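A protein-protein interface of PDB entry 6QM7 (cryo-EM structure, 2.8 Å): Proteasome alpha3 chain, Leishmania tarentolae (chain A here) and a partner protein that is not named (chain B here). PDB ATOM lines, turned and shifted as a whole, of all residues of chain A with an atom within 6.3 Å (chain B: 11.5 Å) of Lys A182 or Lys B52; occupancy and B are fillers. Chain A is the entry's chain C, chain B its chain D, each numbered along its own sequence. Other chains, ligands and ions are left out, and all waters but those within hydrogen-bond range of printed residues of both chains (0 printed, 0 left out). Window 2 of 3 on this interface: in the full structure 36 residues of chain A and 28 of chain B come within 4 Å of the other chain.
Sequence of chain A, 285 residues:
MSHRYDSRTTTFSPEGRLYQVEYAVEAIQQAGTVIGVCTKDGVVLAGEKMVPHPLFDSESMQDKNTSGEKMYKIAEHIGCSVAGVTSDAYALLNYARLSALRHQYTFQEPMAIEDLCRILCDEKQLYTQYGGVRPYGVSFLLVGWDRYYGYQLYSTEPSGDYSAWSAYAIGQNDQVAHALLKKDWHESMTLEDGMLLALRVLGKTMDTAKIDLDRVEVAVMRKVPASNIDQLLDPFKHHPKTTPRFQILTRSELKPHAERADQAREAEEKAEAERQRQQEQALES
Of the 11 printed residues of chain A, 4 touch a printed residue of chain B. Printed residues of chain A that touch a printed residue of chain B: Ser A166, His A178, Leu A181 and Lys A182. Hydrophobic or aromatic side chains of chain A that line the printed part of chain B: Leu A181. Hydrophobic or aromatic side chains of chain B that line the printed part of chain A: Leu B53. Among the printed residues, 7 pairs touch across the chains. Among the printed residues, no Asp or Glu carboxylate lies within 4 Å of a Lys or Arg side-chain nitrogen of the other chain.
The backbone NH of Ser A166 sits at hydrogen-bond distance from the backbone carbonyl oxygen of Leu B53 (2.5 Å).
Among the printed residues, merely in contact across the chains: Ser A166 with Asp B55 (3.5 Å), Ser A166 with Gln B54 (3.5 Å), Lys A182 with Lys B52 (3.6 Å), His A178 with Leu B53 (3.6 Å), Lys A182 with Leu B53 (3.8 Å) and Leu A181 with Leu B53 (3.8 Å).
Of chain B, only Lys B52 (3.6 Å) and Leu B53 (3.8 Å) come within 4 Å of Lys A182. Lys B52 touches one residue of chain A. Ala A179 touches none of the printed residues of chain B. Leu A181 touches just one residue of chain B: Leu B53. No residue of chain B comes within 4 Å of Trp A185. Of the printed residues of chain B, Ser A166 touches Leu B53, Gln B54 and Asp B55. Of the printed residues of chain A, Gln B54 touches Ser A166 (3.5 Å). Printed residues of chain A within 4 Å of Leu B53: Ser A166 (2.5 Å), His A178 (3.6 Å), Leu A181 (3.8 Å) and Lys A182 (3.8 Å). Printed residues of chain B within 4 Å of His A178: Leu B53 (3.6 Å). Of the printed residues of chain A, Asp B55 touches Ser A166 (3.5 Å). Ser B49 touches none of the printed residues of chain A. Asp A184 touches none of the printed residues of chain B. The nearest residue of chain A that does not touch Lys B52 is Ser A166 (4.2 Å).
The side-chain carboxylate of Asp B55 lies within salt-bridge range of the guanidinium group of Arg B57 (3.6 Å).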
ATOM      1  N   SER A 166      22.838  -7.942   6.075  1.00  0.00           N
ATOM      2  CA  SER A 166      22.993  -6.534   5.646  1.00  0.00           C
ATOM      3  C   SER A 166      21.598  -5.908   5.639  1.00  0.00           C
ATOM      4  O   SER A 166      21.428  -4.814   6.194  1.00  0.00           O
ATOM      5  CB  SER A 166      23.640  -6.450   4.297  1.00  0.00           C
ATOM      6  OG  SER A 166      24.614  -7.467   4.105  1.00  0.00           O
ATOM      7  N   GLN A 175       9.563 -13.420   1.969  1.00  0.00           N
ATOM      8  CA  GLN A 175      10.182 -13.857   0.686  1.00  0.00           C
ATOM      9  C   GLN A 175      10.117 -12.719  -0.337  1.00  0.00           C
ATOM     10  O   GLN A 175      11.133 -12.489  -1.022  1.00  0.00           O
ATOM     11  CB  GLN A 175       9.485 -15.102   0.129  1.00  0.00           C
ATOM     12  CG  GLN A 175       9.435 -16.287   1.092  1.00  0.00           C
ATOM     13  CD  GLN A 175      10.727 -17.062   1.206  1.00  0.00           C
ATOM     14  OE1 GLN A 175      10.720 -18.257   1.486  1.00  0.00           O
ATOM     15  NE2 GLN A 175      11.853 -16.399   0.992  1.00  0.00           N
ATOM     16  N   ALA A 177       9.843  -9.529   0.330  1.00  0.00           N
ATOM     17  CA  ALA A 177      10.737  -8.492   0.897  1.00  0.00           C
ATOM     18  C   ALA A 177      12.192  -8.800   0.530  1.00  0.00           C
ATOM     19  O   ALA A 177      12.854  -7.887   0.002  1.00  0.00           O
ATOM     20  CB  ALA A 177      10.564  -8.400   2.390  1.00  0.00           C
ATOM     21  N   HIS A 178      12.660 -10.030   0.780  1.00  0.00           N
ATOM     22  CA  HIS A 178      14.050 -10.497   0.497  1.00  0.00           C
ATOM     23  C   HIS A 178      14.428 -10.218  -0.965  1.00  0.00           C
ATOM     24  O   HIS A 178      15.583  -9.837  -1.199  1.00  0.00           O
ATOM     25  CB  HIS A 178      14.236 -11.989   0.826  1.00  0.00           C
ATOM     26  CG  HIS A 178      14.179 -12.310   2.281  1.00  0.00           C
ATOM     27  ND1 HIS A 178      13.963 -13.596   2.744  1.00  0.00           N
ATOM     28  CD2 HIS A 178      14.263 -11.522   3.379  1.00  0.00           C
ATOM     29  CE1 HIS A 178      13.933 -13.588   4.063  1.00  0.00           C
ATOM     30  NE2 HIS A 178      14.113 -12.327   4.477  1.00  0.00           N
ATOM     31  N   ALA A 179      13.498 -10.412  -1.904  1.00  0.00           N
ATOM     32  CA  ALA A 179      13.661 -10.113  -3.348  1.00  0.00           C
ATOM     33  C   ALA A 179      13.902  -8.612  -3.552  1.00  0.00           C
ATOM     34  O   ALA A 179      14.832  -8.252  -4.296  1.00  0.00           O
ATOM     35  CB  ALA A 179      12.438 -10.569  -4.105  1.00  0.00           C
ATOM     36  N   LEU A 180      13.090  -7.775  -2.902  1.00  0.00           N
ATOM     37  CA  LEU A 180      13.077  -6.296  -3.071  1.00  0.00           C
ATOM     38  C   LEU A 180      14.234  -5.643  -2.301  1.00  0.00           C
ATOM     39  O   LEU A 180      14.558  -4.480  -2.618  1.00  0.00           O
ATOM     40  CB  LEU A 180      11.728  -5.744  -2.597  1.00  0.00           C
ATOM     41  CG  LEU A 180      10.669  -5.567  -3.682  1.00  0.00           C
ATOM     42  CD1 LEU A 180      10.042  -6.898  -4.090  1.00  0.00           C
ATOM     43  CD2 LEU A 180       9.597  -4.594  -3.217  1.00  0.00           C
ATOM     44  N   LEU A 181      14.804  -6.336  -1.315  1.00  0.00           N
ATOM     45  CA  LEU A 181      16.030  -5.896  -0.599  1.00  0.00           C
ATOM     46  C   LEU A 181      17.265  -6.302  -1.411  1.00  0.00           C
ATOM     47  O   LEU A 181      18.187  -5.472  -1.496  1.00  0.00           O
ATOM     48  CB  LEU A 181      16.068  -6.519   0.798  1.00  0.00           C
ATOM     49  CG  LEU A 181      15.077  -5.941   1.806  1.00  0.00           C
ATOM     50  CD1 LEU A 181      14.956  -6.857   3.019  1.00  0.00           C
ATOM     51  CD2 LEU A 181      15.473  -4.529   2.218  1.00  0.00           C
ATOM     52  N   LYS A 182      17.292  -7.528  -1.954  1.00  0.00           N
ATOM     53  CA  LYS A 182      18.399  -8.062  -2.805  1.00  0.00           C
ATOM     54  C   LYS A 182      18.713  -7.077  -3.931  1.00  0.00           C
ATOM     55  O   LYS A 182      19.911  -6.840  -4.199  1.00  0.00           O
ATOM     56  CB  LYS A 182      18.047  -9.407  -3.453  1.00  0.00           C
ATOM     57  CG  LYS A 182      18.657 -10.642  -2.798  1.00  0.00           C
ATOM     58  CD  LYS A 182      19.001 -11.761  -3.782  1.00  0.00           C
ATOM     59  CE  LYS A 182      17.826 -12.241  -4.615  1.00  0.00           C
ATOM     60  NZ  LYS A 182      16.712 -12.746  -3.774  1.00  0.00           N
ATOM     61  N   LYS A 183      17.666  -6.538  -4.558  1.00  0.00           N
ATOM     62  CA  LYS A 183      17.757  -5.638  -5.734  1.00  0.00           C
ATOM     63  C   LYS A 183      18.378  -4.291  -5.324  1.00  0.00           C
ATOM     64  O   LYS A 183      19.318  -3.848  -6.018  1.00  0.00           O
ATOM     65  CB  LYS A 183      16.364  -5.475  -6.345  1.00  0.00           C
ATOM     66  CG  LYS A 183      16.328  -4.970  -7.783  1.00  0.00           C
ATOM     67  CD  LYS A 183      14.938  -4.589  -8.257  1.00  0.00           C
ATOM     68  CE  LYS A 183      13.917  -5.697  -8.087  1.00  0.00           C
ATOM     69  NZ  LYS A 183      12.594  -5.311  -8.633  1.00  0.00           N
ATOM     70  N   ASP A 184      17.902  -3.681  -4.233  1.00  0.00           N
ATOM     71  CA  ASP A 184      18.058  -2.222  -3.970  1.00  0.00           C
ATOM     72  C   ASP A 184      18.999  -1.918  -2.790  1.00  0.00           C
ATOM     73  O   ASP A 184      19.238  -0.715  -2.548  1.00  0.00           O
ATOM     74  CB  ASP A 184      16.677  -1.584  -3.787  1.00  0.00           C
ATOM     75  CG  ASP A 184      15.992  -1.276  -5.108  1.00  0.00           C
ATOM     76  OD1 ASP A 184      15.605  -0.107  -5.310  1.00  0.00           O
ATOM     77  OD2 ASP A 184      15.865  -2.206  -5.931  1.00  0.00           O
ATOM     78  N   TRP A 185      19.533  -2.925  -2.091  1.00  0.00           N
ATOM     79  CA  TRP A 185      20.506  -2.719  -0.984  1.00  0.00           C
ATOM     80  C   TRP A 185      21.927  -2.693  -1.549  1.00  0.00           C
ATOM     81  O   TRP A 185      22.289  -3.668  -2.241  1.00  0.00           O
ATOM     82  CB  TRP A 185      20.382  -3.798   0.101  1.00  0.00           C
ATOM     83  CG  TRP A 185      21.263  -3.492   1.272  1.00  0.00           C
ATOM     84  CD1 TRP A 185      20.944  -2.732   2.358  1.00  0.00           C
ATOM     85  CD2 TRP A 185      22.640  -3.867   1.439  1.00  0.00           C
ATOM     86  NE1 TRP A 185      22.016  -2.631   3.202  1.00  0.00           N
ATOM     87  CE2 TRP A 185      23.072  -3.318   2.666  1.00  0.00           C
ATOM     88  CE3 TRP A 185      23.546  -4.617   0.677  1.00  0.00           C
ATOM     89  CZ2 TRP A 185      24.373  -3.483   3.136  1.00  0.00           C
ATOM     90  CZ3 TRP A 185      24.828  -4.795   1.150  1.00  0.00           C
ATOM     91  CH2 TRP A 185      25.234  -4.234   2.365  1.00  0.00           C
ATOM     92  N   LYS B  48      25.768 -22.169   2.211  1.00  0.00           N
ATOM     93  CA  LYS B  48      24.399 -22.175   1.617  1.00  0.00           C
ATOM     94  C   LYS B  48      24.385 -21.414   0.277  1.00  0.00           C
ATOM     95  O   LYS B  48      23.429 -21.639  -0.492  1.00  0.00           O
ATOM     96  CB  LYS B  48      23.388 -21.605   2.623  1.00  0.00           C
ATOM     97  CG  LYS B  48      23.579 -20.138   2.997  1.00  0.00           C
ATOM     98  CD  LYS B  48      23.097 -19.771   4.393  1.00  0.00           C
ATOM     99  CE  LYS B  48      23.407 -18.334   4.771  1.00  0.00           C
ATOM    100  NZ  LYS B  48      22.721 -17.918   6.018  1.00  0.00           N
ATOM    101  N   SER B  49      25.379 -20.536   0.042  1.00  0.00           N
ATOM    102  CA  SER B  49      25.738 -19.835  -1.228  1.00  0.00           C
ATOM    103  C   SER B  49      25.521 -18.322  -1.055  1.00  0.00           C
ATOM    104  O   SER B  49      24.584 -17.934  -0.323  1.00  0.00           O
ATOM    105  CB  SER B  49      25.019 -20.376  -2.448  1.00  0.00           C
ATOM    106  OG  SER B  49      25.636 -19.915  -3.641  1.00  0.00           O
ATOM    107  N   ALA B  50      26.369 -17.511  -1.703  1.00  0.00           N
ATOM    108  CA  ALA B  50      26.506 -16.044  -1.502  1.00  0.00           C
ATOM    109  C   ALA B  50      25.195 -15.326  -1.860  1.00  0.00           C
ATOM    110  O   ALA B  50      25.026 -14.937  -3.038  1.00  0.00           O
ATOM    111  CB  ALA B  50      27.672 -15.509  -2.308  1.00  0.00           C
ATOM    112  N   VAL B  51      24.305 -15.167  -0.872  1.00  0.00           N
ATOM    113  CA  VAL B  51      23.088 -14.299  -0.941  1.00  0.00           C
ATOM    114  C   VAL B  51      23.562 -12.855  -0.723  1.00  0.00           C
ATOM    115  O   VAL B  51      24.358 -12.648   0.212  1.00  0.00           O
ATOM    116  CB  VAL B  51      22.022 -14.714   0.097  1.00  0.00           C
ATOM    117  CG1 VAL B  51      20.713 -13.959  -0.107  1.00  0.00           C
ATOM    118  CG2 VAL B  51      21.775 -16.220   0.103  1.00  0.00           C
ATOM    119  N   LYS B  52      23.107 -11.897  -1.542  1.00  0.00           N
ATOM    120  CA  LYS B  52      23.574 -10.477  -1.517  1.00  0.00           C
ATOM    121  C   LYS B  52      23.369  -9.852  -0.129  1.00  0.00           C
ATOM    122  O   LYS B  52      24.067  -8.862   0.179  1.00  0.00           O
ATOM    123  CB  LYS B  52      22.833  -9.621  -2.550  1.00  0.00           C
ATOM    124  CG  LYS B  52      23.178  -9.900  -4.007  1.00  0.00           C
ATOM    125  CD  LYS B  52      22.897  -8.725  -4.933  1.00  0.00           C
ATOM    126  CE  LYS B  52      22.720  -9.126  -6.384  1.00  0.00           C
ATOM    127  NZ  LYS B  52      21.381  -9.712  -6.636  1.00  0.00           N
ATOM    128  N   LEU B  53      22.442 -10.403   0.662  1.00  0.00           N
ATOM    129  CA  LEU B  53      21.936  -9.815   1.929  1.00  0.00           C
ATOM    130  C   LEU B  53      22.774 -10.237   3.138  1.00  0.00           C
ATOM    131  O   LEU B  53      22.841  -9.430   4.073  1.00  0.00           O
ATOM    132  CB  LEU B  53      20.482 -10.247   2.115  1.00  0.00           C
ATOM    133  CG  LEU B  53      19.504  -9.717   1.070  1.00  0.00           C
ATOM    134  CD1 LEU B  53      18.077 -10.141   1.410  1.00  0.00           C
ATOM    135  CD2 LEU B  53      19.617  -8.200   0.943  1.00  0.00           C
ATOM    136  N   GLN B  54      23.333 -11.454   3.166  1.00  0.00           N
ATOM    137  CA  GLN B  54      24.126 -11.937   4.333  1.00  0.00           C
ATOM    138  C   GLN B  54      25.343 -11.020   4.488  1.00  0.00           C
ATOM    139  O   GLN B  54      25.949 -10.661   3.459  1.00  0.00           O
ATOM    140  CB  GLN B  54      24.509 -13.418   4.247  1.00  0.00           C
ATOM    141  CG  GLN B  54      25.272 -13.817   2.990  1.00  0.00           C
ATOM    142  CD  GLN B  54      26.318 -14.877   3.244  1.00  0.00           C
ATOM    143  OE1 GLN B  54      26.100 -15.824   3.999  1.00  0.00           O
ATOM    144  NE2 GLN B  54      27.470 -14.725   2.605  1.00  0.00           N
ATOM    145  N   ASP B  55      25.640 -10.630   5.732  1.00  0.00           N
ATOM    146  CA  ASP B  55      26.618  -9.565   6.072  1.00  0.00           C
ATOM    147  C   ASP B  55      27.938  -9.876   5.357  1.00  0.00           C
ATOM    148  O   ASP B  55      28.403 -11.039   5.456  1.00  0.00           O
ATOM    149  CB  ASP B  55      26.792  -9.427   7.586  1.00  0.00           C
ATOM    150  CG  ASP B  55      27.331  -8.084   8.066  1.00  0.00           C
ATOM    151  OD1 ASP B  55      27.771  -8.025   9.229  1.00  0.00           O
ATOM    152  OD2 ASP B  55      27.294  -7.107   7.289  1.00  0.00           O
ATOM    153  N   SER B  56      28.478  -8.888   4.630  1.00  0.00           N
ATOM    154  CA  SER B  56      29.772  -8.954   3.899  1.00  0.00           C
ATOM    155  C   SER B  56      30.886  -9.377   4.866  1.00  0.00           C
ATOM    156  O   SER B  56      31.761 -10.160   4.437  1.00  0.00           O
ATOM    157  CB  SER B  56      30.083  -7.641   3.217  1.00  0.00           C
ATOM    158  OG  SER B  56      29.957  -6.554   4.123  1.00  0.00           O
ATOM    159  N   ARG B  57      30.832  -8.890   6.117  1.00  0.00           N
ATOM    160  CA  ARG B  57      31.728  -9.283   7.244  1.00  0.00           C
ATOM    161  C   ARG B  57      31.759 -10.812   7.350  1.00  0.00           C
ATOM    162  O   ARG B  57      30.676 -11.432   7.319  1.00  0.00           O
ATOM    163  CB  ARG B  57      31.263  -8.631   8.552  1.00  0.00           C
ATOM    164  CG  ARG B  57      32.156  -8.908   9.758  1.00  0.00           C
ATOM    165  CD  ARG B  57      31.599  -9.940  10.729  1.00  0.00           C
ATOM    166  NE  ARG B  57      30.270  -9.591  11.224  1.00  0.00           N
ATOM    167  CZ  ARG B  57      29.550 -10.301  12.093  1.00  0.00           C
ATOM    168  NH1 ARG B  57      30.013 -11.432  12.603  1.00  0.00           N
ATOM    169  NH2 ARG B  57      28.354  -9.861  12.447  1.00  0.00           N
ATOM    170  N   ARG B 202      32.414 -20.161  -4.933  1.00  0.00           N
ATOM    171  CA  ARG B 202      32.021 -19.206  -3.852  1.00  0.00           C
ATOM    172  C   ARG B 202      31.458 -19.935  -2.621  1.00  0.00           C
ATOM    173  O   ARG B 202      31.628 -19.392  -1.506  1.00  0.00           O
ATOM    174  CB  ARG B 202      30.994 -18.176  -4.345  1.00  0.00           C
ATOM    175  CG  ARG B 202      29.734 -18.763  -4.972  1.00  0.00           C
ATOM    176  CD  ARG B 202      29.648 -18.514  -6.468  1.00  0.00           C
ATOM    177  NE  ARG B 202      28.743 -19.432  -7.150  1.00  0.00           N
ATOM    178  CZ  ARG B 202      28.270 -19.277  -8.390  1.00  0.00           C
ATOM    179  NH1 ARG B 202      27.453 -20.188  -8.898  1.00  0.00           N
ATOM    180  NH2 ARG B 202      28.597 -18.220  -9.120  1.00  0.00           N
